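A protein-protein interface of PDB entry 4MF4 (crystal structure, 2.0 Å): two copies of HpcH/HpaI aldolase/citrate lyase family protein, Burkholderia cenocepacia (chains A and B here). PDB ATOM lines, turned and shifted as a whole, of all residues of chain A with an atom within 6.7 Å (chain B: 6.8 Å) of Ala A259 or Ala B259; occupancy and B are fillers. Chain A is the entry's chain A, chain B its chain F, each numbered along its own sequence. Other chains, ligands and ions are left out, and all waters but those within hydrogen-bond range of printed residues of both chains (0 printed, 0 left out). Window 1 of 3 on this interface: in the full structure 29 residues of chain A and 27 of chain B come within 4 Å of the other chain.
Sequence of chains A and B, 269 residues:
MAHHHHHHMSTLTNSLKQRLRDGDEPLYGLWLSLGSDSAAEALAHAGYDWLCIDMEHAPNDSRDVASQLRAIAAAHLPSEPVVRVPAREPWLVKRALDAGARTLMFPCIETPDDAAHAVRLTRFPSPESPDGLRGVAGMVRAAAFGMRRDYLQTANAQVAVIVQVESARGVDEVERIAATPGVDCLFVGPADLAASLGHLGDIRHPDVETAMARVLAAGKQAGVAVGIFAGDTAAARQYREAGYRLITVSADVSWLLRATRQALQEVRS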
ATOM      1  N   TYR A  48       8.378  -3.809  22.206  1.00  0.00           N
ATOM      2  CA  TYR A  48       8.511  -5.271  22.009  1.00  0.00           C
ATOM      3  C   TYR A  48       9.497  -5.850  23.033  1.00  0.00           C
ATOM      4  O   TYR A  48      10.445  -5.168  23.484  1.00  0.00           O
ATOM      5  CB  TYR A  48       8.971  -5.588  20.586  1.00  0.00           C
ATOM      6  CG  TYR A  48       7.843  -5.470  19.605  1.00  0.00           C
ATOM      7  CD1 TYR A  48       7.445  -4.248  19.123  1.00  0.00           C
ATOM      8  CD2 TYR A  48       7.180  -6.599  19.149  1.00  0.00           C
ATOM      9  CE1 TYR A  48       6.335  -4.142  18.263  1.00  0.00           C
ATOM     10  CE2 TYR A  48       6.113  -6.510  18.274  1.00  0.00           C
ATOM     11  CZ  TYR A  48       5.696  -5.285  17.839  1.00  0.00           C
ATOM     12  OH  TYR A  48       4.678  -5.221  16.936  1.00  0.00           O
ATOM     13  N   SER A 254       7.093  -5.211   6.372  1.00  0.00           N
ATOM     14  CA  SER A 254       5.701  -5.589   6.144  1.00  0.00           C
ATOM     15  C   SER A 254       4.729  -4.573   6.776  1.00  0.00           C
ATOM     16  O   SER A 254       3.732  -4.145   6.172  1.00  0.00           O
ATOM     17  CB  SER A 254       5.462  -6.998   6.692  1.00  0.00           C
ATOM     18  OG  SER A 254       6.379  -7.913   6.083  1.00  0.00           O
ATOM     19  N   TRP A 255       5.014  -4.184   8.009  1.00  0.00           N
ATOM     20  CA  TRP A 255       4.163  -3.164   8.673  1.00  0.00           C
ATOM     21  C   TRP A 255       4.232  -1.816   7.981  1.00  0.00           C
ATOM     22  O   TRP A 255       3.201  -1.145   7.848  1.00  0.00           O
ATOM     23  CB  TRP A 255       4.533  -3.000  10.148  1.00  0.00           C
ATOM     24  CG  TRP A 255       4.098  -4.243  10.942  1.00  0.00           C
ATOM     25  CD1 TRP A 255       4.901  -5.116  11.618  1.00  0.00           C
ATOM     26  CD2 TRP A 255       2.762  -4.690  11.156  1.00  0.00           C
ATOM     27  NE1 TRP A 255       4.153  -6.098  12.201  1.00  0.00           N
ATOM     28  CE2 TRP A 255       2.836  -5.870  11.920  1.00  0.00           C
ATOM     29  CE3 TRP A 255       1.509  -4.241  10.715  1.00  0.00           C
ATOM     30  CZ2 TRP A 255       1.727  -6.582  12.293  1.00  0.00           C
ATOM     31  CZ3 TRP A 255       0.387  -4.946  11.110  1.00  0.00           C
ATOM     32  CH2 TRP A 255       0.506  -6.125  11.868  1.00  0.00           C
ATOM     33  N   LEU A 256       5.435  -1.452   7.532  1.00  0.00           N
ATOM     34  CA  LEU A 256       5.643  -0.210   6.816  1.00  0.00           C
ATOM     35  C   LEU A 256       4.814  -0.111   5.553  1.00  0.00           C
ATOM     36  O   LEU A 256       4.158   0.907   5.309  1.00  0.00           O
ATOM     37  CB  LEU A 256       7.142  -0.036   6.468  1.00  0.00           C
ATOM     38  CG  LEU A 256       7.523   1.181   5.649  1.00  0.00           C
ATOM     39  CD1 LEU A 256       7.170   2.473   6.343  1.00  0.00           C
ATOM     40  CD2 LEU A 256       8.999   1.165   5.339  1.00  0.00           C
ATOM     41  N   LEU A 257       4.821  -1.177   4.754  1.00  0.00           N
ATOM     42  CA  LEU A 257       4.006  -1.230   3.553  1.00  0.00           C
ATOM     43  C   LEU A 257       2.514  -1.259   3.879  1.00  0.00           C
ATOM     44  O   LEU A 257       1.720  -0.510   3.291  1.00  0.00           O
ATOM     45  CB  LEU A 257       4.371  -2.459   2.710  1.00  0.00           C
ATOM     46  CG  LEU A 257       5.605  -2.217   1.866  1.00  0.00           C
ATOM     47  CD1 LEU A 257       6.258  -3.519   1.432  1.00  0.00           C
ATOM     48  CD2 LEU A 257       5.271  -1.328   0.664  1.00  0.00           C
ATOM     49  N   ARG A 258       2.119  -2.096   4.812  1.00  0.00           N
ATOM     50  CA  ARG A 258       0.693  -2.218   5.094  1.00  0.00           C
ATOM     51  C   ARG A 258       0.109  -0.862   5.556  1.00  0.00           C
ATOM     52  O   ARG A 258      -0.908  -0.400   5.022  1.00  0.00           O
ATOM     53  CB  ARG A 258       0.424  -3.356   6.095  1.00  0.00           C
ATOM     54  CG  ARG A 258      -1.062  -3.560   6.438  1.00  0.00           C
ATOM     55  CD  ARG A 258      -1.199  -4.575   7.577  1.00  0.00           C
ATOM     56  NE  ARG A 258      -2.564  -4.893   8.002  1.00  0.00           N
ATOM     57  CZ  ARG A 258      -3.325  -5.851   7.456  1.00  0.00           C
ATOM     58  NH1 ARG A 258      -2.915  -6.552   6.404  1.00  0.00           N
ATOM     59  NH2 ARG A 258      -4.527  -6.096   7.949  1.00  0.00           N
ATOM     60  N   ALA A 259       0.762  -0.233   6.531  1.00  0.00           N
ATOM     61  CA  ALA A 259       0.295   1.003   7.102  1.00  0.00           C
ATOM     62  C   ALA A 259       0.293   2.177   6.141  1.00  0.00           C
ATOM     63  O   ALA A 259      -0.679   2.974   6.141  1.00  0.00           O
ATOM     64  CB  ALA A 259       1.110   1.353   8.321  1.00  0.00           C
ATOM     65  N   THR A 260       1.363   2.326   5.353  1.00  0.00           N
ATOM     66  CA  THR A 260       1.395   3.390   4.320  1.00  0.00           C
ATOM     67  C   THR A 260       0.355   3.146   3.240  1.00  0.00           C
ATOM     68  O   THR A 260      -0.303   4.059   2.806  1.00  0.00           O
ATOM     69  CB  THR A 260       2.813   3.606   3.671  1.00  0.00           C
ATOM     70  OG1 THR A 260       3.321   2.387   3.112  1.00  0.00           O
ATOM     71  CG2 THR A 260       3.788   4.095   4.721  1.00  0.00           C
ATOM     72  N   ARG A 261       0.184   1.901   2.794  1.00  0.00           N
ATOM     73  CA  ARG A 261      -0.820   1.653   1.799  1.00  0.00           C
ATOM     74  C   ARG A 261      -2.271   1.925   2.347  1.00  0.00           C
ATOM     75  O   ARG A 261      -3.105   2.534   1.665  1.00  0.00           O
ATOM     76  CB  ARG A 261      -0.687   0.226   1.266  1.00  0.00           C
ATOM     77  CG  ARG A 261       0.519   0.004   0.369  1.00  0.00           C
ATOM     78  CD  ARG A 261       0.445  -1.365  -0.326  1.00  0.00           C
ATOM     79  NE  ARG A 261      -0.529  -1.272  -1.412  1.00  0.00           N
ATOM     80  CZ  ARG A 261      -1.755  -1.785  -1.396  1.00  0.00           C
ATOM     81  NH1 ARG A 261      -2.178  -2.525  -0.366  1.00  0.00           N
ATOM     82  NH2 ARG A 261      -2.570  -1.584  -2.440  1.00  0.00           N
ATOM     83  N   GLN A 262      -2.510   1.516   3.588  1.00  0.00           N
ATOM     84  CA  GLN A 262      -3.786   1.763   4.273  1.00  0.00           C
ATOM     85  C   GLN A 262      -4.095   3.267   4.410  1.00  0.00           C
ATOM     86  O   GLN A 262      -5.199   3.726   4.114  1.00  0.00           O
ATOM     87  CB  GLN A 262      -3.813   1.045   5.644  1.00  0.00           C
ATOM     88  CG  GLN A 262      -5.049   1.276   6.492  1.00  0.00           C
ATOM     89  CD  GLN A 262      -6.349   0.789   5.848  1.00  0.00           C
ATOM     90  OE1 GLN A 262      -6.350  -0.124   5.019  1.00  0.00           O
ATOM     91  NE2 GLN A 262      -7.462   1.366   6.267  1.00  0.00           N
ATOM     92  N   ALA A 263      -3.102   4.032   4.812  1.00  0.00           N
ATOM     93  CA  ALA A 263      -3.263   5.485   4.938  1.00  0.00           C
ATOM     94  C   ALA A 263      -3.652   6.177   3.613  1.00  0.00           C
ATOM     95  O   ALA A 263      -4.601   7.004   3.559  1.00  0.00           O
ATOM     96  CB  ALA A 263      -2.014   6.073   5.529  1.00  0.00           C
ATOM     97  N   LEU A 264      -3.006   5.768   2.534  1.00  0.00           N
ATOM     98  CA  LEU A 264      -3.314   6.287   1.198  1.00  0.00           C
ATOM     99  C   LEU A 264      -4.768   6.005   0.818  1.00  0.00           C
ATOM    100  O   LEU A 264      -5.497   6.905   0.361  1.00  0.00           O
ATOM    101  CB  LEU A 264      -2.399   5.652   0.151  1.00  0.00           C
ATOM    102  CG  LEU A 264      -2.495   6.249  -1.234  1.00  0.00           C
ATOM    103  CD1 LEU A 264      -2.358   7.760  -1.166  1.00  0.00           C
ATOM    104  CD2 LEU A 264      -1.429   5.636  -2.119  1.00  0.00           C
ATOM    105  N   TYR B  48       2.042   5.785  -4.068  1.00  0.00           N
ATOM    106  CA  TYR B  48       2.057   7.228  -3.905  1.00  0.00           C
ATOM    107  C   TYR B  48       2.427   7.963  -5.207  1.00  0.00           C
ATOM    108  O   TYR B  48       3.155   7.457  -6.059  1.00  0.00           O
ATOM    109  CB  TYR B  48       2.941   7.682  -2.743  1.00  0.00           C
ATOM    110  CG  TYR B  48       2.326   7.423  -1.390  1.00  0.00           C
ATOM    111  CD1 TYR B  48       2.242   6.145  -0.872  1.00  0.00           C
ATOM    112  CD2 TYR B  48       1.785   8.456  -0.643  1.00  0.00           C
ATOM    113  CE1 TYR B  48       1.620   5.908   0.351  1.00  0.00           C
ATOM    114  CE2 TYR B  48       1.180   8.235   0.584  1.00  0.00           C
ATOM    115  CZ  TYR B  48       1.086   6.960   1.079  1.00  0.00           C
ATOM    116  OH  TYR B  48       0.475   6.757   2.300  1.00  0.00           O
ATOM    117  N   THR B 233      -4.091  10.911   8.712  1.00  0.00           N
ATOM    118  CA  THR B 233      -5.051  10.862   7.579  1.00  0.00           C
ATOM    119  C   THR B 233      -6.260  11.817   7.721  1.00  0.00           C
ATOM    120  O   THR B 233      -6.734  12.346   6.726  1.00  0.00           O
ATOM    121  CB  THR B 233      -5.609   9.439   7.308  1.00  0.00           C
ATOM    122  OG1 THR B 233      -6.354   8.970   8.433  1.00  0.00           O
ATOM    123  CG2 THR B 233      -4.501   8.476   7.000  1.00  0.00           C
ATOM    124  N   SER B 254       6.948   7.459  11.048  1.00  0.00           N
ATOM    125  CA  SER B 254       5.723   7.666  11.837  1.00  0.00           C
ATOM    126  C   SER B 254       4.743   6.540  11.591  1.00  0.00           C
ATOM    127  O   SER B 254       4.150   5.987  12.542  1.00  0.00           O
ATOM    128  CB  SER B 254       5.079   9.035  11.497  1.00  0.00           C
ATOM    129  OG  SER B 254       6.055  10.077  11.546  1.00  0.00           O
ATOM    130  N   TRP B 255       4.580   6.164  10.315  1.00  0.00           N
ATOM    131  CA  TRP B 255       3.745   5.000  10.003  1.00  0.00           C
ATOM    132  C   TRP B 255       4.340   3.695  10.542  1.00  0.00           C
ATOM    133  O   TRP B 255       3.623   2.825  10.990  1.00  0.00           O
ATOM    134  CB  TRP B 255       3.485   4.878   8.501  1.00  0.00           C
ATOM    135  CG  TRP B 255       2.656   5.981   8.020  1.00  0.00           C
ATOM    136  CD1 TRP B 255       3.012   6.974   7.111  1.00  0.00           C
ATOM    137  CD2 TRP B 255       1.337   6.287   8.445  1.00  0.00           C
ATOM    138  NE1 TRP B 255       1.973   7.851   6.946  1.00  0.00           N
ATOM    139  CE2 TRP B 255       0.937   7.466   7.761  1.00  0.00           C
ATOM    140  CE3 TRP B 255       0.432   5.671   9.308  1.00  0.00           C
ATOM    141  CZ2 TRP B 255      -0.304   7.999   7.908  1.00  0.00           C
ATOM    142  CZ3 TRP B 255      -0.796   6.234   9.482  1.00  0.00           C
ATOM    143  CH2 TRP B 255      -1.150   7.409   8.805  1.00  0.00           C
ATOM    144  N   LEU B 256       5.652   3.559  10.460  1.00  0.00           N
ATOM    145  CA  LEU B 256       6.296   2.364  10.945  1.00  0.00           C
ATOM    146  C   LEU B 256       6.041   2.177  12.464  1.00  0.00           C
ATOM    147  O   LEU B 256       5.727   1.095  12.914  1.00  0.00           O
ATOM    148  CB  LEU B 256       7.798   2.422  10.657  1.00  0.00           C
ATOM    149  CG  LEU B 256       8.580   1.243  11.216  1.00  0.00           C
ATOM    150  CD1 LEU B 256       8.131  -0.070  10.585  1.00  0.00           C
ATOM    151  CD2 LEU B 256      10.061   1.487  11.035  1.00  0.00           C
ATOM    152  N   LEU B 257       6.201   3.257  13.212  1.00  0.00           N
ATOM    153  CA  LEU B 257       5.958   3.248  14.649  1.00  0.00           C
ATOM    154  C   LEU B 257       4.491   3.058  14.999  1.00  0.00           C
ATOM    155  O   LEU B 257       4.169   2.281  15.890  1.00  0.00           O
ATOM    156  CB  LEU B 257       6.476   4.551  15.250  1.00  0.00           C
ATOM    157  CG  LEU B 257       7.944   4.478  15.618  1.00  0.00           C
ATOM    158  CD1 LEU B 257       8.449   5.897  15.884  1.00  0.00           C
ATOM    159  CD2 LEU B 257       8.107   3.610  16.862  1.00  0.00           C
ATOM    160  N   ARG B 258       3.580   3.731  14.292  1.00  0.00           N
ATOM    161  CA  ARG B 258       2.154   3.575  14.620  1.00  0.00           C
ATOM    162  C   ARG B 258       1.719   2.130  14.431  1.00  0.00           C
ATOM    163  O   ARG B 258       1.086   1.522  15.310  1.00  0.00           O
ATOM    164  CB  ARG B 258       1.275   4.437  13.722  1.00  0.00           C
ATOM    165  CG  ARG B 258       1.383   5.918  14.008  1.00  0.00           C
ATOM    166  CD  ARG B 258       0.808   6.761  12.851  1.00  0.00           C
ATOM    167  NE  ARG B 258       0.965   8.191  13.154  1.00  0.00           N
ATOM    168  CZ  ARG B 258       1.204   9.170  12.280  1.00  0.00           C
ATOM    169  NH1 ARG B 258       1.360   8.947  10.975  1.00  0.00           N
ATOM    170  NH2 ARG B 258       1.334  10.407  12.746  1.00  0.00           N
ATOM    171  N   ALA B 259       2.030   1.588  13.249  1.00  0.00           N
ATOM    172  CA  ALA B 259       1.554   0.255  12.895  1.00  0.00           C
ATOM    173  C   ALA B 259       2.135  -0.856  13.775  1.00  0.00           C
ATOM    174  O   ALA B 259       1.391  -1.754  14.198  1.00  0.00           O
ATOM    175  CB  ALA B 259       1.790  -0.035  11.444  1.00  0.00           C
ATOM    176  N   THR B 260       3.424  -0.776  14.105  1.00  0.00           N
ATOM    177  CA  THR B 260       4.044  -1.821  14.919  1.00  0.00           C
ATOM    178  C   THR B 260       3.526  -1.756  16.356  1.00  0.00           C
ATOM    179  O   THR B 260       3.292  -2.788  16.979  1.00  0.00           O
ATOM    180  CB  THR B 260       5.612  -1.752  14.891  1.00  0.00           C
ATOM    181  OG1 THR B 260       6.075  -0.452  15.253  1.00  0.00           O
ATOM    182  CG2 THR B 260       6.130  -2.077  13.525  1.00  0.00           C
ATOM    183  N   ARG B 261       3.379  -0.568  16.918  1.00  0.00           N
ATOM    184  CA  ARG B 261       2.816  -0.431  18.272  1.00  0.00           C
ATOM    185  C   ARG B 261       1.338  -0.821  18.345  1.00  0.00           C
ATOM    186  O   ARG B 261       0.924  -1.441  19.302  1.00  0.00           O
ATOM    187  CB  ARG B 261       2.994   1.003  18.779  1.00  0.00           C
ATOM    188  CG  ARG B 261       4.447   1.410  18.981  1.00  0.00           C
ATOM    189  CD  ARG B 261       4.547   2.783  19.625  1.00  0.00           C
ATOM    190  NE  ARG B 261       3.727   2.796  20.819  1.00  0.00           N
ATOM    191  CZ  ARG B 261       4.143   2.558  22.058  1.00  0.00           C
ATOM    192  NH1 ARG B 261       5.434   2.367  22.354  1.00  0.00           N
ATOM    193  NH2 ARG B 261       3.245   2.576  23.025  1.00  0.00           N
ATOM    194  N   GLN B 262       0.543  -0.472  17.326  1.00  0.00           N
ATOM    195  CA  GLN B 262      -0.866  -0.908  17.278  1.00  0.00           C
ATOM    196  C   GLN B 262      -0.989  -2.426  17.188  1.00  0.00           C
ATOM    197  O   GLN B 262      -1.828  -3.030  17.869  1.00  0.00           O
ATOM    198  CB  GLN B 262      -1.654  -0.257  16.114  1.00  0.00           C
ATOM    199  N   ALA B 263      -0.148  -3.050  16.353  1.00  0.00           N
ATOM    200  CA  ALA B 263      -0.184  -4.512  16.210  1.00  0.00           C
ATOM    201  C   ALA B 263       0.153  -5.195  17.527  1.00  0.00           C
ATOM    202  O   ALA B 263      -0.523  -6.176  17.927  1.00  0.00           O
ATOM    203  CB  ALA B 263       0.694  -4.975  15.072  1.00  0.00           C
ATOM    204  N   LEU B 264       1.122  -4.649  18.257  1.00  0.00           N
ATOM    205  CA  LEU B 264       1.486  -5.241  19.545  1.00  0.00           C
ATOM    206  C   LEU B 264       0.335  -5.211  20.564  1.00  0.00           C
ATOM    207  O   LEU B 264       0.014  -6.235  21.184  1.00  0.00           O
ATOM    208  CB  LEU B 264       2.739  -4.606  20.118  1.00  0.00           C
ATOM    209  CG  LEU B 264       3.191  -5.186  21.468  1.00  0.00           C
ATOM    210  CD1 LEU B 264       3.318  -6.704  21.416  1.00  0.00           C
ATOM    211  CD2 LEU B 264       4.537  -4.561  21.835  1.00  0.00           C
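Of the printed residues of chain B, Ala A259 touches Trp B255 and Ala B259. Of the printed residues of chain A, Ala B259 touches Ala A259. Printed residues of chain A within 4 Å of Thr B260: Tyr A48 and Trp A255. Of the printed residues of chain B, Thr A260 touches Tyr B48 (2.9 Å) and Trp B255 (3.8 Å). Of the printed residues of chain B, Tyr A48 touches Thr B260 and Leu B264. Printed residues of chain B within 4 Å of Leu A264: Tyr B48. Gln A262 touches none of the printed residues of chain B. Gln B262 touches none of the printed residues of chain A. The nearest printed residue of chain A that does not touch Thr B233 is Leu A264 (5.4 Å).
The side-chain hydroxyl (OH) of Tyr A48 lies within hydrogen-bond range of the backbone carbonyl oxygen (O) of Thr B260 (2.8 Å). O of Thr A260 is in hydrogen-bond range of OH of Tyr B48, at 2.9 Å.
OG1 of Thr A260 is in hydrogen-bond range of O of Leu A256 (2.8 Å). The backbone carbonyl oxygen (O) of Leu A257 is in hydrogen-bond range of the side-chain hydroxyl (OG1) of Thr A260 (3.3 Å). O of Leu B256 lies within hydrogen-bond range of OG1 of Thr B260, 2.8 Å away. The backbone carbonyl oxygen (O) of Leu B257 sits at hydrogen-bond distance from the side-chain hydroxyl (OG1) of Thr B260 (3.4 Å).
Among the printed residues, merely in contact across the chains: Trp A255 with Ala B263 (3.4 Å), Ala A259 with Ala B259 (3.5 Å), Ala A263 with Trp B255 (3.5 Å), Leu A264 with Tyr B48 (3.6 Å), Ala A263 with Thr B233 (3.7 Å), Tyr A48 with Leu B264 (3.8 Å), Trp A255 with Thr B260 (3.8 Å), Thr A260 with Trp B255 (3.8 Å) and Ala A259 with Trp B255 (3.95 Å).
Tyr A48 touches Leu B264, and with the chains exchanged Leu A264 touches Tyr B48. Trp A255 touches Thr B260, and with the chains exchanged Thr A260 touches Trp B255. Trp A255 touches Ala B263, and with the chains exchanged Ala A263 touches Trp B255. Ala A259 touches its own counterpart, Ala B259. Positions printed for both chains: 48, 254, 255, 256, 257, 258, 259, 260, 261, 262, 263 and 264. Of the 11 pairs that touch across the chains among the printed residues, 9 have their exchanged pair printed and touching as well.
Of the 12 printed residues of chain A, 6 touch a printed residue of chain B. Of the 13 printed residues of chain B, 7 touch a printed residue of chain A. Printed residues of chain B that touch a printed residue of chain A: Tyr B48, Thr B233, Trp B255, Ala B259, Thr B260, Ala B263 and Leu B264. Hydrophobic or aromatic side chains of chain B that line the printed part of chain A: Tyr B48, Trp B255, Ala B259, Ala B263 and Leu B264. Among the printed residues, 11 pairs touch across the chains. Among the printed residues, no Asp or Glu carboxylate lies within 4 Å of a Lys or Arg side-chain nitrogen of the other chain.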
